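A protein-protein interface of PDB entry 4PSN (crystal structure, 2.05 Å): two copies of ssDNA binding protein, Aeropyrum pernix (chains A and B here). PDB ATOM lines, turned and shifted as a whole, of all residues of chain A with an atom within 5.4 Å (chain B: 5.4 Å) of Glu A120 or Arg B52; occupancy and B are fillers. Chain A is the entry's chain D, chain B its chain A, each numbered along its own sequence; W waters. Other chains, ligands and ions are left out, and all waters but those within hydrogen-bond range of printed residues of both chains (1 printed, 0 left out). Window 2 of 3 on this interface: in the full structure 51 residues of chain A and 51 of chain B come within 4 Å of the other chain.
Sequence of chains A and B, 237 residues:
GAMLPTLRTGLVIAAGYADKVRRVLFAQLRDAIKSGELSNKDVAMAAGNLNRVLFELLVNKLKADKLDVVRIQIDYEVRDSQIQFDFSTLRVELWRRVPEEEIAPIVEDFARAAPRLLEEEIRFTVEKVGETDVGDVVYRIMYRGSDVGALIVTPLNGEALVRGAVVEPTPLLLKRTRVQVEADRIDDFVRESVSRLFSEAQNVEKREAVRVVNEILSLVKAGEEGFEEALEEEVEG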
ATOM      1  N   ARG A 116      13.192  22.954   8.267  1.00  0.00           N
ATOM      2  CA  ARG A 116      14.096  21.975   8.851  1.00  0.00           C
ATOM      3  C   ARG A 116      13.812  21.794  10.347  1.00  0.00           C
ATOM      4  O   ARG A 116      13.547  20.680  10.822  1.00  0.00           O
ATOM      5  CB  ARG A 116      15.534  22.424   8.643  1.00  0.00           C
ATOM      6  CG  ARG A 116      16.532  21.291   8.575  1.00  0.00           C
ATOM      7  CD  ARG A 116      17.619  21.505   9.600  1.00  0.00           C
ATOM      8  NE  ARG A 116      17.948  22.920   9.730  1.00  0.00           N
ATOM      9  CZ  ARG A 116      18.534  23.451  10.796  1.00  0.00           C
ATOM     10  NH1 ARG A 116      18.796  24.751  10.832  1.00  0.00           N
ATOM     11  NH2 ARG A 116      18.851  22.678  11.828  1.00  0.00           N
ATOM     12  N   LEU A 117      13.864  22.900  11.082  1.00  0.00           N
ATOM     13  CA  LEU A 117      13.618  22.884  12.520  1.00  0.00           C
ATOM     14  C   LEU A 117      12.299  22.199  12.898  1.00  0.00           C
ATOM     15  O   LEU A 117      12.215  21.538  13.932  1.00  0.00           O
ATOM     16  CB  LEU A 117      13.651  24.311  13.082  1.00  0.00           C
ATOM     17  CG  LEU A 117      15.002  24.829  13.569  1.00  0.00           C
ATOM     18  CD1 LEU A 117      16.112  24.302  12.692  1.00  0.00           C
ATOM     19  CD2 LEU A 117      15.012  26.349  13.612  1.00  0.00           C
ATOM     20  N   LEU A 118      11.271  22.374  12.072  1.00  0.00           N
ATOM     21  CA  LEU A 118       9.970  21.771  12.333  1.00  0.00           C
ATOM     22  C   LEU A 118      10.124  20.288  12.664  1.00  0.00           C
ATOM     23  O   LEU A 118       9.485  19.777  13.583  1.00  0.00           O
ATOM     24  CB  LEU A 118       9.048  21.920  11.116  1.00  0.00           C
ATOM     25  CG  LEU A 118       7.818  22.832  11.146  1.00  0.00           C
ATOM     26  CD1 LEU A 118       6.677  22.226  10.308  1.00  0.00           C
ATOM     27  CD2 LEU A 118       7.354  23.130  12.565  1.00  0.00           C
ATOM     28  N   GLU A 119      10.991  19.608  11.919  1.00  0.00           N
ATOM     29  CA  GLU A 119      11.059  18.148  11.959  1.00  0.00           C
ATOM     30  C   GLU A 119      12.247  17.612  12.748  1.00  0.00           C
ATOM     31  O   GLU A 119      12.174  16.538  13.354  1.00  0.00           O
ATOM     32  CB  GLU A 119      11.099  17.595  10.532  1.00  0.00           C
ATOM     33  CG  GLU A 119       9.858  17.898   9.706  1.00  0.00           C
ATOM     34  CD  GLU A 119       8.643  17.108  10.164  1.00  0.00           C
ATOM     35  OE1 GLU A 119       8.516  16.846  11.381  1.00  0.00           O
ATOM     36  OE2 GLU A 119       7.819  16.739   9.300  1.00  0.00           O
ATOM     37  N   GLU A 120      13.338  18.370  12.722  1.00  0.00           N
ATOM     38  CA  GLU A 120      14.608  17.976  13.328  1.00  0.00           C
ATOM     39  C   GLU A 120      14.517  17.685  14.837  1.00  0.00           C
ATOM     40  O   GLU A 120      13.894  18.436  15.587  1.00  0.00           O
ATOM     41  CB  GLU A 120      15.622  19.078  13.056  1.00  0.00           C
ATOM     42  CG  GLU A 120      17.032  18.776  13.465  1.00  0.00           C
ATOM     43  CD  GLU A 120      17.956  19.911  13.087  1.00  0.00           C
ATOM     44  OE1 GLU A 120      18.095  20.855  13.893  1.00  0.00           O
ATOM     45  OE2 GLU A 120      18.520  19.870  11.972  1.00  0.00           O
ATOM     46  N   GLU A 121      15.153  16.595  15.264  1.00  0.00           N
ATOM     47  CA  GLU A 121      15.071  16.105  16.641  1.00  0.00           C
ATOM     48  C   GLU A 121      15.759  17.038  17.629  1.00  0.00           C
ATOM     49  O   GLU A 121      16.854  17.525  17.367  1.00  0.00           O
ATOM     50  CB  GLU A 121      15.714  14.721  16.730  1.00  0.00           C
ATOM     51  CG  GLU A 121      15.613  14.046  18.087  1.00  0.00           C
ATOM     52  CD  GLU A 121      16.458  12.779  18.168  1.00  0.00           C
ATOM     53  OE1 GLU A 121      17.590  12.778  17.633  1.00  0.00           O
ATOM     54  OE2 GLU A 121      15.991  11.782  18.761  1.00  0.00           O
ATOM     55  N   ILE A 122      15.127  17.277  18.775  1.00  0.00           N
ATOM     56  CA  ILE A 122      15.716  18.158  19.786  1.00  0.00           C
ATOM     57  C   ILE A 122      16.764  17.411  20.607  1.00  0.00           C
ATOM     58  O   ILE A 122      16.509  16.313  21.099  1.00  0.00           O
ATOM     59  CB  ILE A 122      14.632  18.759  20.719  1.00  0.00           C
ATOM     60  CG1 ILE A 122      13.599  19.524  19.888  1.00  0.00           C
ATOM     61  CG2 ILE A 122      15.258  19.702  21.745  1.00  0.00           C
ATOM     62  CD1 ILE A 122      12.206  19.555  20.516  1.00  0.00           C
ATOM     63  N   TYR A 143      18.443  22.366  27.796  1.00  0.00           N
ATOM     64  CA  TYR A 143      18.488  22.633  26.372  1.00  0.00           C
ATOM     65  C   TYR A 143      19.544  23.720  26.168  1.00  0.00           C
ATOM     66  O   TYR A 143      19.427  24.814  26.724  1.00  0.00           O
ATOM     67  CB  TYR A 143      17.118  23.093  25.860  1.00  0.00           C
ATOM     68  CG  TYR A 143      17.088  23.331  24.369  1.00  0.00           C
ATOM     69  CD1 TYR A 143      17.462  22.324  23.478  1.00  0.00           C
ATOM     70  CD2 TYR A 143      16.700  24.556  23.845  1.00  0.00           C
ATOM     71  CE1 TYR A 143      17.448  22.532  22.112  1.00  0.00           C
ATOM     72  CE2 TYR A 143      16.671  24.772  22.467  1.00  0.00           C
ATOM     73  CZ  TYR A 143      17.054  23.761  21.608  1.00  0.00           C
ATOM     74  OH  TYR A 143      17.035  23.973  20.237  1.00  0.00           O
ATOM     75  N   PRO A 169      12.483  23.630  24.235  1.00  0.00           N
ATOM     76  CA  PRO A 169      11.971  24.694  23.363  1.00  0.00           C
ATOM     77  C   PRO A 169      10.504  24.520  22.989  1.00  0.00           C
ATOM     78  O   PRO A 169       9.930  25.435  22.414  1.00  0.00           O
ATOM     79  CB  PRO A 169      12.848  24.570  22.116  1.00  0.00           C
ATOM     80  CG  PRO A 169      13.204  23.145  22.077  1.00  0.00           C
ATOM     81  CD  PRO A 169      13.385  22.729  23.501  1.00  0.00           C
ATOM     82  N   THR A 170       9.926  23.362  23.296  1.00  0.00           N
ATOM     83  CA  THR A 170       8.478  23.186  23.233  1.00  0.00           C
ATOM     84  C   THR A 170       8.067  22.254  24.384  1.00  0.00           C
ATOM     85  O   THR A 170       8.827  21.374  24.755  1.00  0.00           O
ATOM     86  CB  THR A 170       8.026  22.644  21.859  1.00  0.00           C
ATOM     87  OG1 THR A 170       6.614  22.825  21.717  1.00  0.00           O
ATOM     88  CG2 THR A 170       8.372  21.164  21.691  1.00  0.00           C
ATOM     89  N   TYR B  17       3.113  32.413  24.855  1.00  0.00           N
ATOM     90  CA  TYR B  17       2.784  32.289  23.432  1.00  0.00           C
ATOM     91  C   TYR B  17       2.476  30.856  23.019  1.00  0.00           C
ATOM     92  O   TYR B  17       1.617  30.641  22.178  1.00  0.00           O
ATOM     93  CB  TYR B  17       3.885  32.866  22.524  1.00  0.00           C
ATOM     94  CG  TYR B  17       5.027  31.898  22.272  1.00  0.00           C
ATOM     95  CD1 TYR B  17       4.923  30.903  21.310  1.00  0.00           C
ATOM     96  CD2 TYR B  17       6.203  31.977  23.007  1.00  0.00           C
ATOM     97  CE1 TYR B  17       5.957  30.012  21.088  1.00  0.00           C
ATOM     98  CE2 TYR B  17       7.244  31.083  22.794  1.00  0.00           C
ATOM     99  CZ  TYR B  17       7.113  30.106  21.832  1.00  0.00           C
ATOM    100  OH  TYR B  17       8.143  29.222  21.613  1.00  0.00           O
ATOM    101  N   ALA B  47       1.170  22.086  16.422  1.00  0.00           N
ATOM    102  CA  ALA B  47       1.385  23.211  17.330  1.00  0.00           C
ATOM    103  C   ALA B  47       2.745  23.111  18.044  1.00  0.00           C
ATOM    104  O   ALA B  47       3.466  24.112  18.191  1.00  0.00           O
ATOM    105  CB  ALA B  47       0.262  23.298  18.339  1.00  0.00           C
ATOM    106  N   GLY B  48       3.094  21.904  18.473  1.00  0.00           N
ATOM    107  CA  GLY B  48       4.350  21.663  19.165  1.00  0.00           C
ATOM    108  C   GLY B  48       5.542  21.996  18.299  1.00  0.00           C
ATOM    109  O   GLY B  48       6.490  22.640  18.760  1.00  0.00           O
ATOM    110  N   ASN B  49       5.498  21.558  17.041  1.00  0.00           N
ATOM    111  CA  ASN B  49       6.574  21.860  16.103  1.00  0.00           C
ATOM    112  C   ASN B  49       6.644  23.355  15.789  1.00  0.00           C
ATOM    113  O   ASN B  49       7.729  23.932  15.718  1.00  0.00           O
ATOM    114  CB  ASN B  49       6.445  21.017  14.824  1.00  0.00           C
ATOM    115  CG  ASN B  49       6.651  19.516  15.081  1.00  0.00           C
ATOM    116  OD1 ASN B  49       7.270  19.117  16.071  1.00  0.00           O
ATOM    117  ND2 ASN B  49       6.128  18.687  14.190  1.00  0.00           N
ATOM    118  N   LEU B  50       5.491  23.998  15.634  1.00  0.00           N
ATOM    119  CA  LEU B  50       5.505  25.430  15.375  1.00  0.00           C
ATOM    120  C   LEU B  50       6.113  26.161  16.571  1.00  0.00           C
ATOM    121  O   LEU B  50       6.917  27.078  16.404  1.00  0.00           O
ATOM    122  CB  LEU B  50       4.101  25.961  15.071  1.00  0.00           C
ATOM    123  CG  LEU B  50       4.060  27.464  14.804  1.00  0.00           C
ATOM    124  CD1 LEU B  50       4.836  27.802  13.521  1.00  0.00           C
ATOM    125  CD2 LEU B  50       2.625  27.969  14.706  1.00  0.00           C
ATOM    126  N   ASN B  51       5.740  25.738  17.778  1.00  0.00           N
ATOM    127  CA  ASN B  51       6.224  26.387  18.994  1.00  0.00           C
ATOM    128  C   ASN B  51       7.732  26.283  19.146  1.00  0.00           C
ATOM    129  O   ASN B  51       8.384  27.201  19.657  1.00  0.00           O
ATOM    130  CB  ASN B  51       5.515  25.840  20.246  1.00  0.00           C
ATOM    131  CG  ASN B  51       4.123  26.448  20.438  1.00  0.00           C
ATOM    132  OD1 ASN B  51       3.196  25.792  20.927  1.00  0.00           O
ATOM    133  ND2 ASN B  51       3.972  27.704  20.027  1.00  0.00           N
ATOM    134  N   ARG B  52       8.273  25.155  18.697  1.00  0.00           N
ATOM    135  CA  ARG B  52       9.704  24.904  18.740  1.00  0.00           C
ATOM    136  C   ARG B  52      10.393  25.911  17.824  1.00  0.00           C
ATOM    137  O   ARG B  52      11.396  26.530  18.184  1.00  0.00           O
ATOM    138  CB  ARG B  52       9.976  23.463  18.291  1.00  0.00           C
ATOM    139  CG  ARG B  52      11.377  22.987  18.503  1.00  0.00           C
ATOM    140  CD  ARG B  52      12.258  23.355  17.335  1.00  0.00           C
ATOM    141  NE  ARG B  52      13.667  23.119  17.642  1.00  0.00           N
ATOM    142  CZ  ARG B  52      14.334  22.020  17.309  1.00  0.00           C
ATOM    143  NH1 ARG B  52      13.731  21.042  16.637  1.00  0.00           N
ATOM    144  NH2 ARG B  52      15.610  21.905  17.645  1.00  0.00           N
ATOM    145  N   VAL B  53       9.831  26.103  16.641  1.00  0.00           N
ATOM    146  CA  VAL B  53      10.395  27.072  15.706  1.00  0.00           C
ATOM    147  C   VAL B  53      10.297  28.496  16.273  1.00  0.00           C
ATOM    148  O   VAL B  53      11.241  29.283  16.181  1.00  0.00           O
ATOM    149  CB  VAL B  53       9.669  27.008  14.356  1.00  0.00           C
ATOM    150  CG1 VAL B  53      10.167  28.100  13.429  1.00  0.00           C
ATOM    151  CG2 VAL B  53       9.849  25.639  13.734  1.00  0.00           C
ATOM    152  N   LEU B  54       9.143  28.825  16.850  1.00  0.00           N
ATOM    153  CA  LEU B  54       8.936  30.153  17.414  1.00  0.00           C
ATOM    154  C   LEU B  54       9.891  30.421  18.572  1.00  0.00           C
ATOM    155  O   LEU B  54      10.369  31.535  18.735  1.00  0.00           O
ATOM    156  CB  LEU B  54       7.487  30.349  17.846  1.00  0.00           C
ATOM    157  CG  LEU B  54       6.492  30.374  16.690  1.00  0.00           C
ATOM    158  CD1 LEU B  54       5.060  30.252  17.209  1.00  0.00           C
ATOM    159  CD2 LEU B  54       6.683  31.637  15.861  1.00  0.00           C
ATOM    160  N   PHE B  55      10.186  29.394  19.365  1.00  0.00           N
ATOM    161  CA  PHE B  55      11.149  29.549  20.450  1.00  0.00           C
ATOM    162  C   PHE B  55      12.521  30.038  19.960  1.00  0.00           C
ATOM    163  O   PHE B  55      13.118  30.941  20.553  1.00  0.00           O
ATOM    164  CB  PHE B  55      11.322  28.239  21.222  1.00  0.00           C
ATOM    165  CG  PHE B  55      12.248  28.360  22.386  1.00  0.00           C
ATOM    166  CD1 PHE B  55      11.786  28.830  23.603  1.00  0.00           C
ATOM    167  CD2 PHE B  55      13.583  28.041  22.261  1.00  0.00           C
ATOM    168  CE1 PHE B  55      12.642  28.955  24.668  1.00  0.00           C
ATOM    169  CE2 PHE B  55      14.441  28.166  23.329  1.00  0.00           C
ATOM    170  CZ  PHE B  55      13.972  28.621  24.530  1.00  0.00           C
ATOM    171  N   GLU B  56      13.034  29.421  18.900  1.00  0.00           N
ATOM    172  CA  GLU B  56      14.356  29.790  18.407  1.00  0.00           C
ATOM    173  C   GLU B  56      14.293  31.232  17.909  1.00  0.00           C
ATOM    174  O   GLU B  56      15.167  32.044  18.207  1.00  0.00           O
ATOM    175  CB  GLU B  56      14.813  28.862  17.277  1.00  0.00           C
ATOM    176  CG  GLU B  56      14.485  27.379  17.484  1.00  0.00           C
ATOM    177  CD  GLU B  56      15.308  26.728  18.590  1.00  0.00           C
ATOM    178  OE1 GLU B  56      16.257  27.371  19.091  1.00  0.00           O
ATOM    179  OE2 GLU B  56      15.003  25.570  18.950  1.00  0.00           O
HETATM  180  O   HOH W   1       7.739  26.924  22.939  1.00  0.00           O
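The side-chain amide oxygen of Asn B49 lies close to the backbone carbonyl oxygen of Leu A118. O of Gly B48 sits at hydrogen-bond distance from OG1 of Thr A170 (3.0 Å). NH1 of Arg B52 is in hydrogen-bond range of O of Glu A120 (2.8 Å). NH1 of Arg B52 is in hydrogen-bond range of O of Leu A117 (3.1 Å). OE2 of Glu B56 lies within hydrogen-bond range of OH of Tyr A143.
OE2 of Glu B56 lies within salt-bridge range of NE of Arg B52, at 3.1 Å. The side-chain hydroxyl (OH) of Tyr B17 lies within hydrogen-bond range of the backbone NH (N) of Phe B55, 3.0 Å away. OH of Tyr B17 sits at hydrogen-bond distance from O of Asn B51. NH2 of Arg A116 is in salt-bridge range of OE2 of Glu A120, at 2.8 Å. O of Ala B47 sits close to OD1 of Asn B51 (3.2 Å).
Among the printed residues, pairs that only touch across the chains: Leu A118 with Leu B50 (3.7 Å), Leu A118 with Val B53 (3.7 Å), Ile A122 with Arg B52 (3.6 Å), Tyr A143 with Arg B52 (3.6 Å), Pro A169 with Asn B51 (3.6 Å), Pro A169 with Arg B52 (3.7 Å), Pro A169 with Phe B55 (3.3 Å), Pro A169 with Glu B56 (3.96 Å) and Thr A170 with Asn B51 (3.5 Å).
Glu A120 touches one residue of chain B. Of the printed residues of chain A, Leu B50 touches Leu A118 (3.7 Å). Printed residues of chain A within 4 Å of Val B53: Leu A118. Printed residues of chain A within 4 Å of Asn B51: Pro A169 and Thr A170. Of the printed residues of chain B, Pro A169 touches Asn B51, Arg B52, Phe B55 and Glu B56. The nearest printed residue of chain B that does not touch Glu A120 is Asn B49 (6.7 Å).
Printed residues of chain A that touch a printed residue of chain B: Leu A117, Leu A118, Glu A120, Ile A122, Tyr A143, Pro A169 and Thr A170. Hydrophobic or aromatic side chains of chain A within 4 Å of the printed part of chain B: Leu A118, Ile A122, Tyr A143 and Pro A169. Hydrophobic or aromatic side chains of chain B within 4 Å of the printed part of chain A: Val B53 and Phe B55. Along chain B the printed residues that touch a printed residue of chain A span positions 48 to 56.
No position is printed for both chains. Of the 14 pairs that touch across the chains among the printed residues, none has its exchanged pair printed and touching as well.
Water W1 lies within hydrogen-bond range of OH of Tyr B17, O of Pro A169 and O of Asn B51.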
